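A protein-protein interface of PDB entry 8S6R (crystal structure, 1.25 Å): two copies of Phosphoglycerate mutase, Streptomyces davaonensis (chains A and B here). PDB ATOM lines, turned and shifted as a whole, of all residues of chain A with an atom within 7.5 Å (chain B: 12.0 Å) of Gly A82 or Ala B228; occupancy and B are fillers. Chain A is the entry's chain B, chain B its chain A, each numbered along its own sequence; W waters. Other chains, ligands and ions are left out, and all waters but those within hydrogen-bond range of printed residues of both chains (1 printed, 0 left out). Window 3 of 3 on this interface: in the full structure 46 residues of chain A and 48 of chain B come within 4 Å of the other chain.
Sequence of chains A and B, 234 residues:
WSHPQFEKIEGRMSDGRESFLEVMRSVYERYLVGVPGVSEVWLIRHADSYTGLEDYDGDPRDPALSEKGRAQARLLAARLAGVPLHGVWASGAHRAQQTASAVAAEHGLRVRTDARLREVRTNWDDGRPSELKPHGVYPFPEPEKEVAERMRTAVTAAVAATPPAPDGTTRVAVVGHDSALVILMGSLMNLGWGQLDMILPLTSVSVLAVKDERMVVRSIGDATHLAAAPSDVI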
ATOM      1  N   TRP A  42      15.119  13.613 -28.214  1.00  0.00           N
ATOM      2  CA  TRP A  42      14.555  13.099 -29.462  1.00  0.00           C
ATOM      3  C   TRP A  42      13.662  14.198 -30.026  1.00  0.00           C
ATOM      4  O   TRP A  42      12.527  14.415 -29.562  1.00  0.00           O
ATOM      5  CB  TRP A  42      13.821  11.765 -29.246  1.00  0.00           C
ATOM      6  CG  TRP A  42      14.814  10.621 -28.965  1.00  0.00           C
ATOM      7  CD1 TRP A  42      16.022  10.740 -28.341  1.00  0.00           C
ATOM      8  CD2 TRP A  42      14.658   9.251 -29.326  1.00  0.00           C
ATOM      9  NE1 TRP A  42      16.626   9.471 -28.280  1.00  0.00           N
ATOM     10  CE2 TRP A  42      15.804   8.563 -28.884  1.00  0.00           C
ATOM     11  CE3 TRP A  42      13.652   8.518 -29.976  1.00  0.00           C
ATOM     12  CZ2 TRP A  42      15.959   7.204 -29.061  1.00  0.00           C
ATOM     13  CZ3 TRP A  42      13.833   7.168 -30.177  1.00  0.00           C
ATOM     14  CH2 TRP A  42      14.956   6.517 -29.685  1.00  0.00           C
ATOM     15  N   ALA A  77       3.940   6.720 -32.595  1.00  0.00           N
ATOM     16  CA  ALA A  77       3.725   6.391 -31.194  1.00  0.00           C
ATOM     17  C   ALA A  77       4.037   4.929 -30.946  1.00  0.00           C
ATOM     18  O   ALA A  77       4.587   4.579 -29.885  1.00  0.00           O
ATOM     19  CB  ALA A  77       2.296   6.767 -30.811  1.00  0.00           C
ATOM     20  N   ALA A  78       3.691   4.055 -31.898  1.00  0.00           N
ATOM     21  CA  ALA A  78       4.043   2.643 -31.757  1.00  0.00           C
ATOM     22  C   ALA A  78       5.550   2.454 -31.785  1.00  0.00           C
ATOM     23  O   ALA A  78       6.092   1.620 -31.045  1.00  0.00           O
ATOM     24  CB  ALA A  78       3.363   1.814 -32.835  1.00  0.00           C
ATOM     25  N   ARG A  79       6.236   3.166 -32.687  1.00  0.00           N
ATOM     26  CA  ARG A  79       7.693   3.060 -32.772  1.00  0.00           C
ATOM     27  C   ARG A  79       8.332   3.455 -31.455  1.00  0.00           C
ATOM     28  O   ARG A  79       9.236   2.763 -30.963  1.00  0.00           O
ATOM     29  CB  ARG A  79       8.197   3.960 -33.908  1.00  0.00           C
ATOM     30  CG  ARG A  79       9.699   4.128 -33.848  1.00  0.00           C
ATOM     31  CD  ARG A  79      10.162   5.168 -34.842  1.00  0.00           C
ATOM     32  NE  ARG A  79      11.590   5.424 -34.680  1.00  0.00           N
ATOM     33  CZ  ARG A  79      12.307   6.131 -35.549  1.00  0.00           C
ATOM     34  NH1 ARG A  79      11.736   6.707 -36.586  1.00  0.00           N
ATOM     35  NH2 ARG A  79      13.614   6.279 -35.340  1.00  0.00           N
ATOM     36  N   LEU A  80       7.826   4.508 -30.821  1.00  0.00           N
ATOM     37  CA  LEU A  80       8.425   5.011 -29.594  1.00  0.00           C
ATOM     38  C   LEU A  80       7.877   4.332 -28.336  1.00  0.00           C
ATOM     39  O   LEU A  80       8.407   4.596 -27.251  1.00  0.00           O
ATOM     40  CB  LEU A  80       8.257   6.534 -29.493  1.00  0.00           C
ATOM     41  CG  LEU A  80       8.982   7.301 -30.628  1.00  0.00           C
ATOM     42  CD1 LEU A  80       8.797   8.807 -30.421  1.00  0.00           C
ATOM     43  CD2 LEU A  80      10.422   6.928 -30.759  1.00  0.00           C
ATOM     44  N   ALA A  81       6.881   3.447 -28.461  1.00  0.00           N
ATOM     45  CA  ALA A  81       6.283   2.843 -27.274  1.00  0.00           C
ATOM     46  C   ALA A  81       7.293   2.051 -26.470  1.00  0.00           C
ATOM     47  O   ALA A  81       7.219   2.030 -25.233  1.00  0.00           O
ATOM     48  CB  ALA A  81       5.146   1.948 -27.697  1.00  0.00           C
ATOM     49  N   GLY A  82       8.233   1.381 -27.143  1.00  0.00           N
ATOM     50  CA  GLY A  82       9.226   0.549 -26.477  1.00  0.00           C
ATOM     51  C   GLY A  82      10.513   1.264 -26.117  1.00  0.00           C
ATOM     52  O   GLY A  82      11.453   0.621 -25.629  1.00  0.00           O
ATOM     53  N   VAL A  83      10.595   2.563 -26.335  1.00  0.00           N
ATOM     54  CA  VAL A  83      11.772   3.355 -26.002  1.00  0.00           C
ATOM     55  C   VAL A  83      11.554   4.001 -24.634  1.00  0.00           C
ATOM     56  O   VAL A  83      10.543   4.697 -24.449  1.00  0.00           O
ATOM     57  CB  VAL A  83      11.952   4.444 -27.076  1.00  0.00           C
ATOM     58  CG1 VAL A  83      13.023   5.391 -26.694  1.00  0.00           C
ATOM     59  CG2 VAL A  83      12.230   3.815 -28.447  1.00  0.00           C
ATOM     60  N   PRO A  84      12.469   3.850 -23.673  1.00  0.00           N
ATOM     61  CA  PRO A  84      12.297   4.577 -22.392  1.00  0.00           C
ATOM     62  C   PRO A  84      12.313   6.072 -22.650  1.00  0.00           C
ATOM     63  O   PRO A  84      13.273   6.598 -23.220  1.00  0.00           O
ATOM     64  CB  PRO A  84      13.513   4.135 -21.574  1.00  0.00           C
ATOM     65  CG  PRO A  84      13.843   2.774 -22.155  1.00  0.00           C
ATOM     66  CD  PRO A  84      13.604   2.905 -23.637  1.00  0.00           C
ATOM     67  N   LEU A  85      11.230   6.747 -22.270  1.00  0.00           N
ATOM     68  CA  LEU A  85      11.097   8.184 -22.427  1.00  0.00           C
ATOM     69  C   LEU A  85      10.700   8.781 -21.094  1.00  0.00           C
ATOM     70  O   LEU A  85       9.858   8.219 -20.388  1.00  0.00           O
ATOM     71  CB  LEU A  85       9.999   8.657 -23.405  1.00  0.00           C
ATOM     72  CG  LEU A  85      10.203   8.396 -24.896  1.00  0.00           C
ATOM     73  CD1 LEU A  85       8.972   8.969 -25.624  1.00  0.00           C
ATOM     74  CD2 LEU A  85      11.504   9.023 -25.414  1.00  0.00           C
ATOM     75  N   GLU A 106       1.707   6.494 -24.643  1.00  0.00           N
ATOM     76  CA  GLU A 106       2.259   5.153 -24.484  1.00  0.00           C
ATOM     77  C   GLU A 106       3.231   5.065 -23.315  1.00  0.00           C
ATOM     78  O   GLU A 106       3.816   3.996 -23.101  1.00  0.00           O
ATOM     79  CB  GLU A 106       2.995   4.735 -25.766  1.00  0.00           C
ATOM     80  CG  GLU A 106       2.160   4.743 -27.036  1.00  0.00           C
ATOM     81  CD  GLU A 106       1.010   3.768 -27.007  1.00  0.00           C
ATOM     82  OE1 GLU A 106       1.152   2.662 -26.441  1.00  0.00           O
ATOM     83  OE2 GLU A 106      -0.051   4.103 -27.574  1.00  0.00           O
ATOM     84  N   HIS A 107       3.429   6.156 -22.574  1.00  0.00           N
ATOM     85  CA  HIS A 107       4.423   6.217 -21.507  1.00  0.00           C
ATOM     86  C   HIS A 107       3.849   6.784 -20.228  1.00  0.00           C
ATOM     87  O   HIS A 107       4.597   6.933 -19.254  1.00  0.00           O
ATOM     88  CB  HIS A 107       5.641   7.055 -21.925  1.00  0.00           C
ATOM     89  CG  HIS A 107       6.283   6.561 -23.181  1.00  0.00           C
ATOM     90  ND1 HIS A 107       7.295   5.628 -23.179  1.00  0.00           N
ATOM     91  CD2 HIS A 107       6.038   6.857 -24.485  1.00  0.00           C
ATOM     92  CE1 HIS A 107       7.647   5.367 -24.427  1.00  0.00           C
ATOM     93  NE2 HIS A 107       6.903   6.096 -25.238  1.00  0.00           N
ATOM     94  N   ARG A 171      15.890  10.427 -21.471  1.00  0.00           N
ATOM     95  CA  ARG A 171      15.506  10.799 -22.829  1.00  0.00           C
ATOM     96  C   ARG A 171      14.277  11.702 -22.740  1.00  0.00           C
ATOM     97  O   ARG A 171      13.296  11.368 -22.061  1.00  0.00           O
ATOM     98  CB  ARG A 171      15.251   9.490 -23.602  1.00  0.00           C
ATOM     99  CG  ARG A 171      14.939   9.589 -25.085  1.00  0.00           C
ATOM    100  CD  ARG A 171      14.900   8.202 -25.720  1.00  0.00           C
ATOM    101  NE  ARG A 171      16.206   7.559 -25.768  1.00  0.00           N
ATOM    102  CZ  ARG A 171      16.589   6.494 -25.069  1.00  0.00           C
ATOM    103  NH1 ARG A 171      15.788   5.892 -24.188  1.00  0.00           N
ATOM    104  NH2 ARG A 171      17.824   6.037 -25.224  1.00  0.00           N
ATOM    105  N   LYS B  68      29.228  -7.970 -28.807  1.00  0.00           N
ATOM    106  CA  LYS B  68      28.407  -6.757 -28.871  1.00  0.00           C
ATOM    107  C   LYS B  68      27.883  -6.537 -30.272  1.00  0.00           C
ATOM    108  O   LYS B  68      26.702  -6.203 -30.467  1.00  0.00           O
ATOM    109  CB  LYS B  68      29.227  -5.568 -28.403  1.00  0.00           C
ATOM    110  CG  LYS B  68      28.453  -4.253 -28.362  1.00  0.00           C
ATOM    111  CD  LYS B  68      29.428  -3.108 -28.130  1.00  0.00           C
ATOM    112  CE  LYS B  68      28.725  -1.833 -27.723  1.00  0.00           C
ATOM    113  NZ  LYS B  68      29.724  -0.762 -27.450  1.00  0.00           N
ATOM    114  N   ALA B  71      24.982  -8.681 -31.256  1.00  0.00           N
ATOM    115  CA  ALA B  71      23.742  -8.238 -30.608  1.00  0.00           C
ATOM    116  C   ALA B  71      23.188  -7.016 -31.339  1.00  0.00           C
ATOM    117  O   ALA B  71      21.973  -6.919 -31.565  1.00  0.00           O
ATOM    118  CB  ALA B  71      24.046  -7.876 -29.159  1.00  0.00           C
ATOM    119  N   GLN B  72      24.053  -6.088 -31.732  1.00  0.00           N
ATOM    120  CA  GLN B  72      23.568  -4.942 -32.495  1.00  0.00           C
ATOM    121  C   GLN B  72      23.004  -5.367 -33.839  1.00  0.00           C
ATOM    122  O   GLN B  72      21.970  -4.863 -34.274  1.00  0.00           O
ATOM    123  CB  GLN B  72      24.689  -3.939 -32.720  1.00  0.00           C
ATOM    124  CG  GLN B  72      25.276  -3.341 -31.441  1.00  0.00           C
ATOM    125  CD  GLN B  72      26.529  -2.508 -31.758  1.00  0.00           C
ATOM    126  OE1 GLN B  72      27.256  -2.745 -32.768  1.00  0.00           O
ATOM    127  NE2 GLN B  72      26.795  -1.513 -30.937  1.00  0.00           N
ATOM    128  N   ARG B  74      21.603  -8.119 -34.584  1.00  0.00           N
ATOM    129  CA  ARG B  74      20.308  -8.759 -34.382  1.00  0.00           C
ATOM    130  C   ARG B  74      19.221  -7.705 -34.254  1.00  0.00           C
ATOM    131  O   ARG B  74      18.132  -7.847 -34.828  1.00  0.00           O
ATOM    132  CB  ARG B  74      20.364  -9.589 -33.108  1.00  0.00           C
ATOM    133  CG  ARG B  74      21.104 -10.912 -33.262  1.00  0.00           C
ATOM    134  CD  ARG B  74      20.770 -11.894 -32.136  1.00  0.00           C
ATOM    135  NE  ARG B  74      20.958 -11.352 -30.789  1.00  0.00           N
ATOM    136  CZ  ARG B  74      22.100 -11.360 -30.106  1.00  0.00           C
ATOM    137  NH1 ARG B  74      23.240 -11.810 -30.638  1.00  0.00           N
ATOM    138  NH2 ARG B  74      22.106 -10.890 -28.864  1.00  0.00           N
ATOM    139  N   LEU B  75      19.489  -6.666 -33.466  1.00  0.00           N
ATOM    140  CA  LEU B  75      18.485  -5.628 -33.278  1.00  0.00           C
ATOM    141  C   LEU B  75      18.220  -4.903 -34.585  1.00  0.00           C
ATOM    142  O   LEU B  75      17.083  -4.564 -34.895  1.00  0.00           O
ATOM    143  CB  LEU B  75      18.946  -4.649 -32.202  1.00  0.00           C
ATOM    144  CG  LEU B  75      18.897  -5.220 -30.786  1.00  0.00           C
ATOM    145  CD1 LEU B  75      19.646  -4.321 -29.835  1.00  0.00           C
ATOM    146  CD2 LEU B  75      17.422  -5.439 -30.351  1.00  0.00           C
ATOM    147  N   LEU B  76      19.268  -4.649 -35.369  1.00  0.00           N
ATOM    148  CA  LEU B  76      19.092  -4.016 -36.675  1.00  0.00           C
ATOM    149  C   LEU B  76      18.297  -4.905 -37.616  1.00  0.00           C
ATOM    150  O   LEU B  76      17.391  -4.431 -38.317  1.00  0.00           O
ATOM    151  CB  LEU B  76      20.469  -3.781 -37.291  1.00  0.00           C
ATOM    152  CG  LEU B  76      20.468  -3.296 -38.745  1.00  0.00           C
ATOM    153  CD1 LEU B  76      19.928  -1.891 -38.836  1.00  0.00           C
ATOM    154  CD2 LEU B  76      21.860  -3.351 -39.339  1.00  0.00           C
ATOM    155  N   ALA B  78      16.131  -7.191 -36.902  1.00  0.00           N
ATOM    156  CA  ALA B  78      14.728  -7.193 -36.486  1.00  0.00           C
ATOM    157  C   ALA B  78      14.031  -5.887 -36.883  1.00  0.00           C
ATOM    158  O   ALA B  78      12.885  -5.903 -37.341  1.00  0.00           O
ATOM    159  CB  ALA B  78      14.622  -7.431 -34.985  1.00  0.00           C
ATOM    160  N   ARG B  79      14.716  -4.760 -36.715  1.00  0.00           N
ATOM    161  CA  ARG B  79      14.156  -3.484 -37.151  1.00  0.00           C
ATOM    162  C   ARG B  79      13.815  -3.505 -38.641  1.00  0.00           C
ATOM    163  O   ARG B  79      12.754  -3.007 -39.040  1.00  0.00           O
ATOM    164  CB  ARG B  79      15.140  -2.358 -36.849  1.00  0.00           C
ATOM    165  CG  ARG B  79      14.742  -1.030 -37.504  1.00  0.00           C
ATOM    166  CD  ARG B  79      15.786   0.027 -37.276  1.00  0.00           C
ATOM    167  NE  ARG B  79      15.474   1.248 -38.021  1.00  0.00           N
ATOM    168  CZ  ARG B  79      16.140   2.386 -37.885  1.00  0.00           C
ATOM    169  NH1 ARG B  79      17.206   2.484 -37.111  1.00  0.00           N
ATOM    170  NH2 ARG B  79      15.744   3.459 -38.583  1.00  0.00           N
ATOM    171  N   LEU B 202      27.333   2.700 -34.909  1.00  0.00           N
ATOM    172  CA  LEU B 202      27.299   1.314 -35.377  1.00  0.00           C
ATOM    173  C   LEU B 202      25.867   0.856 -35.600  1.00  0.00           C
ATOM    174  O   LEU B 202      24.987   1.073 -34.753  1.00  0.00           O
ATOM    175  CB  LEU B 202      28.000   0.380 -34.390  1.00  0.00           C
ATOM    176  CG  LEU B 202      29.479   0.729 -34.230  1.00  0.00           C
ATOM    177  CD1 LEU B 202      29.984   0.099 -32.910  1.00  0.00           C
ATOM    178  CD2 LEU B 202      30.329   0.248 -35.428  1.00  0.00           C
ATOM    179  N   THR B 203      25.636   0.200 -36.732  1.00  0.00           N
ATOM    180  CA  THR B 203      24.309  -0.228 -37.194  1.00  0.00           C
ATOM    181  C   THR B 203      23.340   0.918 -37.471  1.00  0.00           C
ATOM    182  O   THR B 203      22.130   0.671 -37.618  1.00  0.00           O
ATOM    183  CB  THR B 203      23.633  -1.352 -36.402  1.00  0.00           C
ATOM    184  OG1 THR B 203      23.238  -0.903 -35.086  1.00  0.00           O
ATOM    185  CG2 THR B 203      24.538  -2.555 -36.279  1.00  0.00           C
ATOM    186  N   ASP B 222      20.640   7.100 -37.840  1.00  0.00           N
ATOM    187  CA  ASP B 222      19.668   6.641 -36.830  1.00  0.00           C
ATOM    188  C   ASP B 222      19.997   5.209 -36.361  1.00  0.00           C
ATOM    189  O   ASP B 222      19.884   4.256 -37.132  1.00  0.00           O
ATOM    190  CB  ASP B 222      18.259   6.744 -37.415  1.00  0.00           C
ATOM    191  CG  ASP B 222      17.184   6.340 -36.428  1.00  0.00           C
ATOM    192  OD1 ASP B 222      17.213   5.170 -35.956  1.00  0.00           O
ATOM    193  OD2 ASP B 222      16.327   7.177 -36.088  1.00  0.00           O
ATOM    194  N   ALA B 223      20.299   5.068 -35.060  1.00  0.00           N
ATOM    195  CA  ALA B 223      20.520   3.763 -34.437  1.00  0.00           C
ATOM    196  C   ALA B 223      19.531   3.548 -33.291  1.00  0.00           C
ATOM    197  O   ALA B 223      19.858   2.968 -32.242  1.00  0.00           O
ATOM    198  CB  ALA B 223      21.978   3.570 -33.994  1.00  0.00           C
ATOM    199  N   THR B 224      18.320   4.054 -33.480  1.00  0.00           N
ATOM    200  CA  THR B 224      17.338   4.050 -32.408  1.00  0.00           C
ATOM    201  C   THR B 224      16.858   2.654 -32.036  1.00  0.00           C
ATOM    202  O   THR B 224      16.269   2.480 -30.961  1.00  0.00           O
ATOM    203  CB  THR B 224      16.167   4.992 -32.734  1.00  0.00           C
ATOM    204  OG1 THR B 224      15.532   4.612 -33.949  1.00  0.00           O
ATOM    205  CG2 THR B 224      16.557   6.486 -32.761  1.00  0.00           C
ATOM    206  N   HIS B 225      17.096   1.641 -32.884  1.00  0.00           N
ATOM    207  CA  HIS B 225      16.813   0.266 -32.464  1.00  0.00           C
ATOM    208  C   HIS B 225      17.687  -0.202 -31.295  1.00  0.00           C
ATOM    209  O   HIS B 225      17.377  -1.215 -30.691  1.00  0.00           O
ATOM    210  CB  HIS B 225      17.024  -0.708 -33.650  1.00  0.00           C
ATOM    211  CG  HIS B 225      18.342  -0.527 -34.343  1.00  0.00           C
ATOM    212  ND1 HIS B 225      18.542   0.494 -35.248  1.00  0.00           N
ATOM    213  CD2 HIS B 225      19.523  -1.185 -34.213  1.00  0.00           C
ATOM    214  CE1 HIS B 225      19.793   0.416 -35.683  1.00  0.00           C
ATOM    215  NE2 HIS B 225      20.417  -0.562 -35.055  1.00  0.00           N
ATOM    216  N   LEU B 226      18.756   0.524 -30.963  1.00  0.00           N
ATOM    217  CA  LEU B 226      19.578   0.200 -29.808  1.00  0.00           C
ATOM    218  C   LEU B 226      19.096   0.884 -28.532  1.00  0.00           C
ATOM    219  O   LEU B 226      19.668   0.667 -27.471  1.00  0.00           O
ATOM    220  CB  LEU B 226      21.021   0.613 -30.103  1.00  0.00           C
ATOM    221  CG  LEU B 226      21.658  -0.014 -31.344  1.00  0.00           C
ATOM    222  CD1 LEU B 226      23.096   0.495 -31.453  1.00  0.00           C
ATOM    223  CD2 LEU B 226      21.576  -1.535 -31.344  1.00  0.00           C
ATOM    224  N   ALA B 227      18.081   1.753 -28.620  1.00  0.00           N
ATOM    225  CA  ALA B 227      17.724   2.576 -27.460  1.00  0.00           C
ATOM    226  C   ALA B 227      17.289   1.754 -26.266  1.00  0.00           C
ATOM    227  O   ALA B 227      17.617   2.095 -25.125  1.00  0.00           O
ATOM    228  CB  ALA B 227      16.659   3.603 -27.852  1.00  0.00           C
ATOM    229  N   ALA B 228      16.563   0.674 -26.493  1.00  0.00           N
ATOM    230  CA  ALA B 228      16.091  -0.144 -25.377  1.00  0.00           C
ATOM    231  C   ALA B 228      17.098  -1.212 -24.929  1.00  0.00           C
ATOM    232  O   ALA B 228      16.844  -1.915 -23.939  1.00  0.00           O
ATOM    233  CB  ALA B 228      14.740  -0.772 -25.733  1.00  0.00           C
ATOM    234  N   ALA B 229      18.249  -1.303 -25.604  1.00  0.00           N
ATOM    235  CA  ALA B 229      19.192  -2.410 -25.458  1.00  0.00           C
ATOM    236  C   ALA B 229      19.966  -2.325 -24.140  1.00  0.00           C
ATOM    237  O   ALA B 229      19.998  -1.277 -23.488  1.00  0.00           O
ATOM    238  CB  ALA B 229      20.174  -2.375 -26.628  1.00  0.00           C
ATOM    239  N   PRO B 230      20.607  -3.420 -23.729  1.00  0.00           N
ATOM    240  CA  PRO B 230      21.445  -3.378 -22.522  1.00  0.00           C
ATOM    241  C   PRO B 230      22.661  -2.477 -22.714  1.00  0.00           C
ATOM    242  O   PRO B 230      23.006  -2.060 -23.824  1.00  0.00           O
ATOM    243  CB  PRO B 230      21.861  -4.841 -22.328  1.00  0.00           C
ATOM    244  CG  PRO B 230      20.790  -5.625 -23.004  1.00  0.00           C
ATOM    245  CD  PRO B 230      20.408  -4.801 -24.203  1.00  0.00           C
ATOM    246  N   SER B 231      23.318  -2.177 -21.588  1.00  0.00           N
ATOM    247  CA  SER B 231      24.462  -1.268 -21.601  1.00  0.00           C
ATOM    248  C   SER B 231      25.656  -1.854 -22.349  1.00  0.00           C
ATOM    249  O   SER B 231      26.439  -1.104 -22.949  1.00  0.00           O
ATOM    250  CB  SER B 231      24.855  -0.887 -20.168  1.00  0.00           C
ATOM    251  OG  SER B 231      25.403  -1.990 -19.461  1.00  0.00           O
ATOM    252  N   ASP B 232      25.816  -3.179 -22.326  1.00  0.00           N
ATOM    253  CA  ASP B 232      26.891  -3.846 -23.054  1.00  0.00           C
ATOM    254  C   ASP B 232      26.573  -4.053 -24.539  1.00  0.00           C
ATOM    255  O   ASP B 232      27.290  -4.787 -25.227  1.00  0.00           O
ATOM    256  CB  ASP B 232      27.289  -5.160 -22.362  1.00  0.00           C
ATOM    257  CG  ASP B 232      26.136  -6.143 -22.241  1.00  0.00           C
ATOM    258  OD1 ASP B 232      25.016  -5.843 -22.712  1.00  0.00           O
ATOM    259  OD2 ASP B 232      26.358  -7.230 -21.669  1.00  0.00           O
ATOM    260  N   VAL B 233      25.521  -3.415 -25.050  1.00  0.00           N
ATOM    261  CA  VAL B 233      25.137  -3.531 -26.450  1.00  0.00           C
ATOM    262  C   VAL B 233      25.096  -2.184 -27.158  1.00  0.00           C
ATOM    263  O   VAL B 233      25.474  -2.088 -28.330  1.00  0.00           O
ATOM    264  CB  VAL B 233      23.809  -4.299 -26.617  1.00  0.00           C
ATOM    265  CG1 VAL B 233      23.348  -4.284 -28.071  1.00  0.00           C
ATOM    266  CG2 VAL B 233      23.997  -5.732 -26.137  1.00  0.00           C
ATOM    267  N   ILE B 234      24.650  -1.130 -26.476  1.00  0.00           N
ATOM    268  CA  ILE B 234      24.500   0.185 -27.117  1.00  0.00           C
ATOM    269  C   ILE B 234      25.828   0.728 -27.655  1.00  0.00           C
ATOM    270  O   ILE B 234      26.879   0.562 -27.038  1.00  0.00           O
ATOM    271  CB  ILE B 234      23.812   1.204 -26.179  1.00  0.00           C
ATOM    272  CG1 ILE B 234      22.541   0.601 -25.583  1.00  0.00           C
ATOM    273  CG2 ILE B 234      23.481   2.501 -26.930  1.00  0.00           C
ATOM    274  CD1 ILE B 234      21.947   1.415 -24.452  1.00  0.00           C
ATOM    275  OXT ILE B 234      25.888   1.354 -28.719  1.00  0.00           O
HETATM  276  O   HOH W   1      12.890   4.090 -32.455  1.00  0.00           O
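The guanidinium group (NH2) of Arg A79 is in salt-bridge range of the side-chain carboxylate (OD2) of Asp B222.
The guanidinium group of Arg A79 is in hydrogen-bond range of the side-chain hydroxyl of Thr B224, 2.9 Å away.
The guanidinium group (NH1) of Arg B79 lies within salt-bridge range of the side-chain carboxylate (OD1) of Asp B222, 2.9 Å away.
The side-chain carboxylate (OD1) of Asp B222 lies within hydrogen-bond range of the side-chain hydroxyl (OG1) of Thr B224 (2.7 Å).
The backbone carbonyl oxygen (O) of Pro A84 sits at hydrogen-bond distance from the guanidinium group (NH1) of Arg A171, 2.8 Å away.
Among the printed residues, merely in contact across the chains: Trp A42 with Thr B224 (3.5 Å), Trp A42 with Ala B227 (3.8 Å), Gly A82 with Ala B228 (3.6 Å) and Arg A171 with Ala B227 (3.8 Å).
Of the printed residues of chain B, Gly A82 touches Ala B228.
Ala B228 touches just one residue of chain A: Gly A82.
No residue of chain B comes within 4 Å of Ala A78.
No residue of chain B comes within 4 Å of Ala A81.
No residue of chain B comes within 4 Å of Val A83.
No residue of chain B comes within 4 Å of Pro A84.
Printed residues of chain A within 4 Å of Asp B222: Arg A79 (3.0 Å).
Printed residues of chain A within 4 Å of Ala B227: Trp A42 and Arg A171.
Printed residues of chain B within 4 Å of Arg A171: Ala B227 (3.8 Å).
Of the printed residues of chain B, Trp A42 touches Thr B224 (3.5 Å) and Ala B227 (3.8 Å).
Printed residues of chain B within 4 Å of Arg A79: Asp B222 (3.0 Å) and Thr B224 (2.9 Å).
Ala B223 touches none of the printed residues of chain A.
Arg B74 touches none of the printed residues of chain A.
The nearest residue of chain A that does not touch Ala B228 is Pro A84 (4.3 Å).
Of the 23 printed residues of chain B, 4 touch a printed residue of chain A.
Printed residues of chain B that touch a printed residue of chain A: Asp B222, Thr B224, Ala B227 and Ala B228.
Hydrophobic or aromatic side chains of chain B that line the printed part of chain A: Ala B227 and Ala B228.
Of the 13 printed residues of chain A, 4 touch a printed residue of chain B.
Printed residues of chain A that touch a printed residue of chain B: Trp A42, Arg A79, Gly A82 and Arg A171.
Hydrophobic or aromatic side chains of chain A within 4 Å of the printed part of chain B: Trp A42.
2 positions are printed for both chains.
Water W1 lies within hydrogen-bond range of the guanidinium group of Arg A79 and the side-chain hydroxyl of Thr B224.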
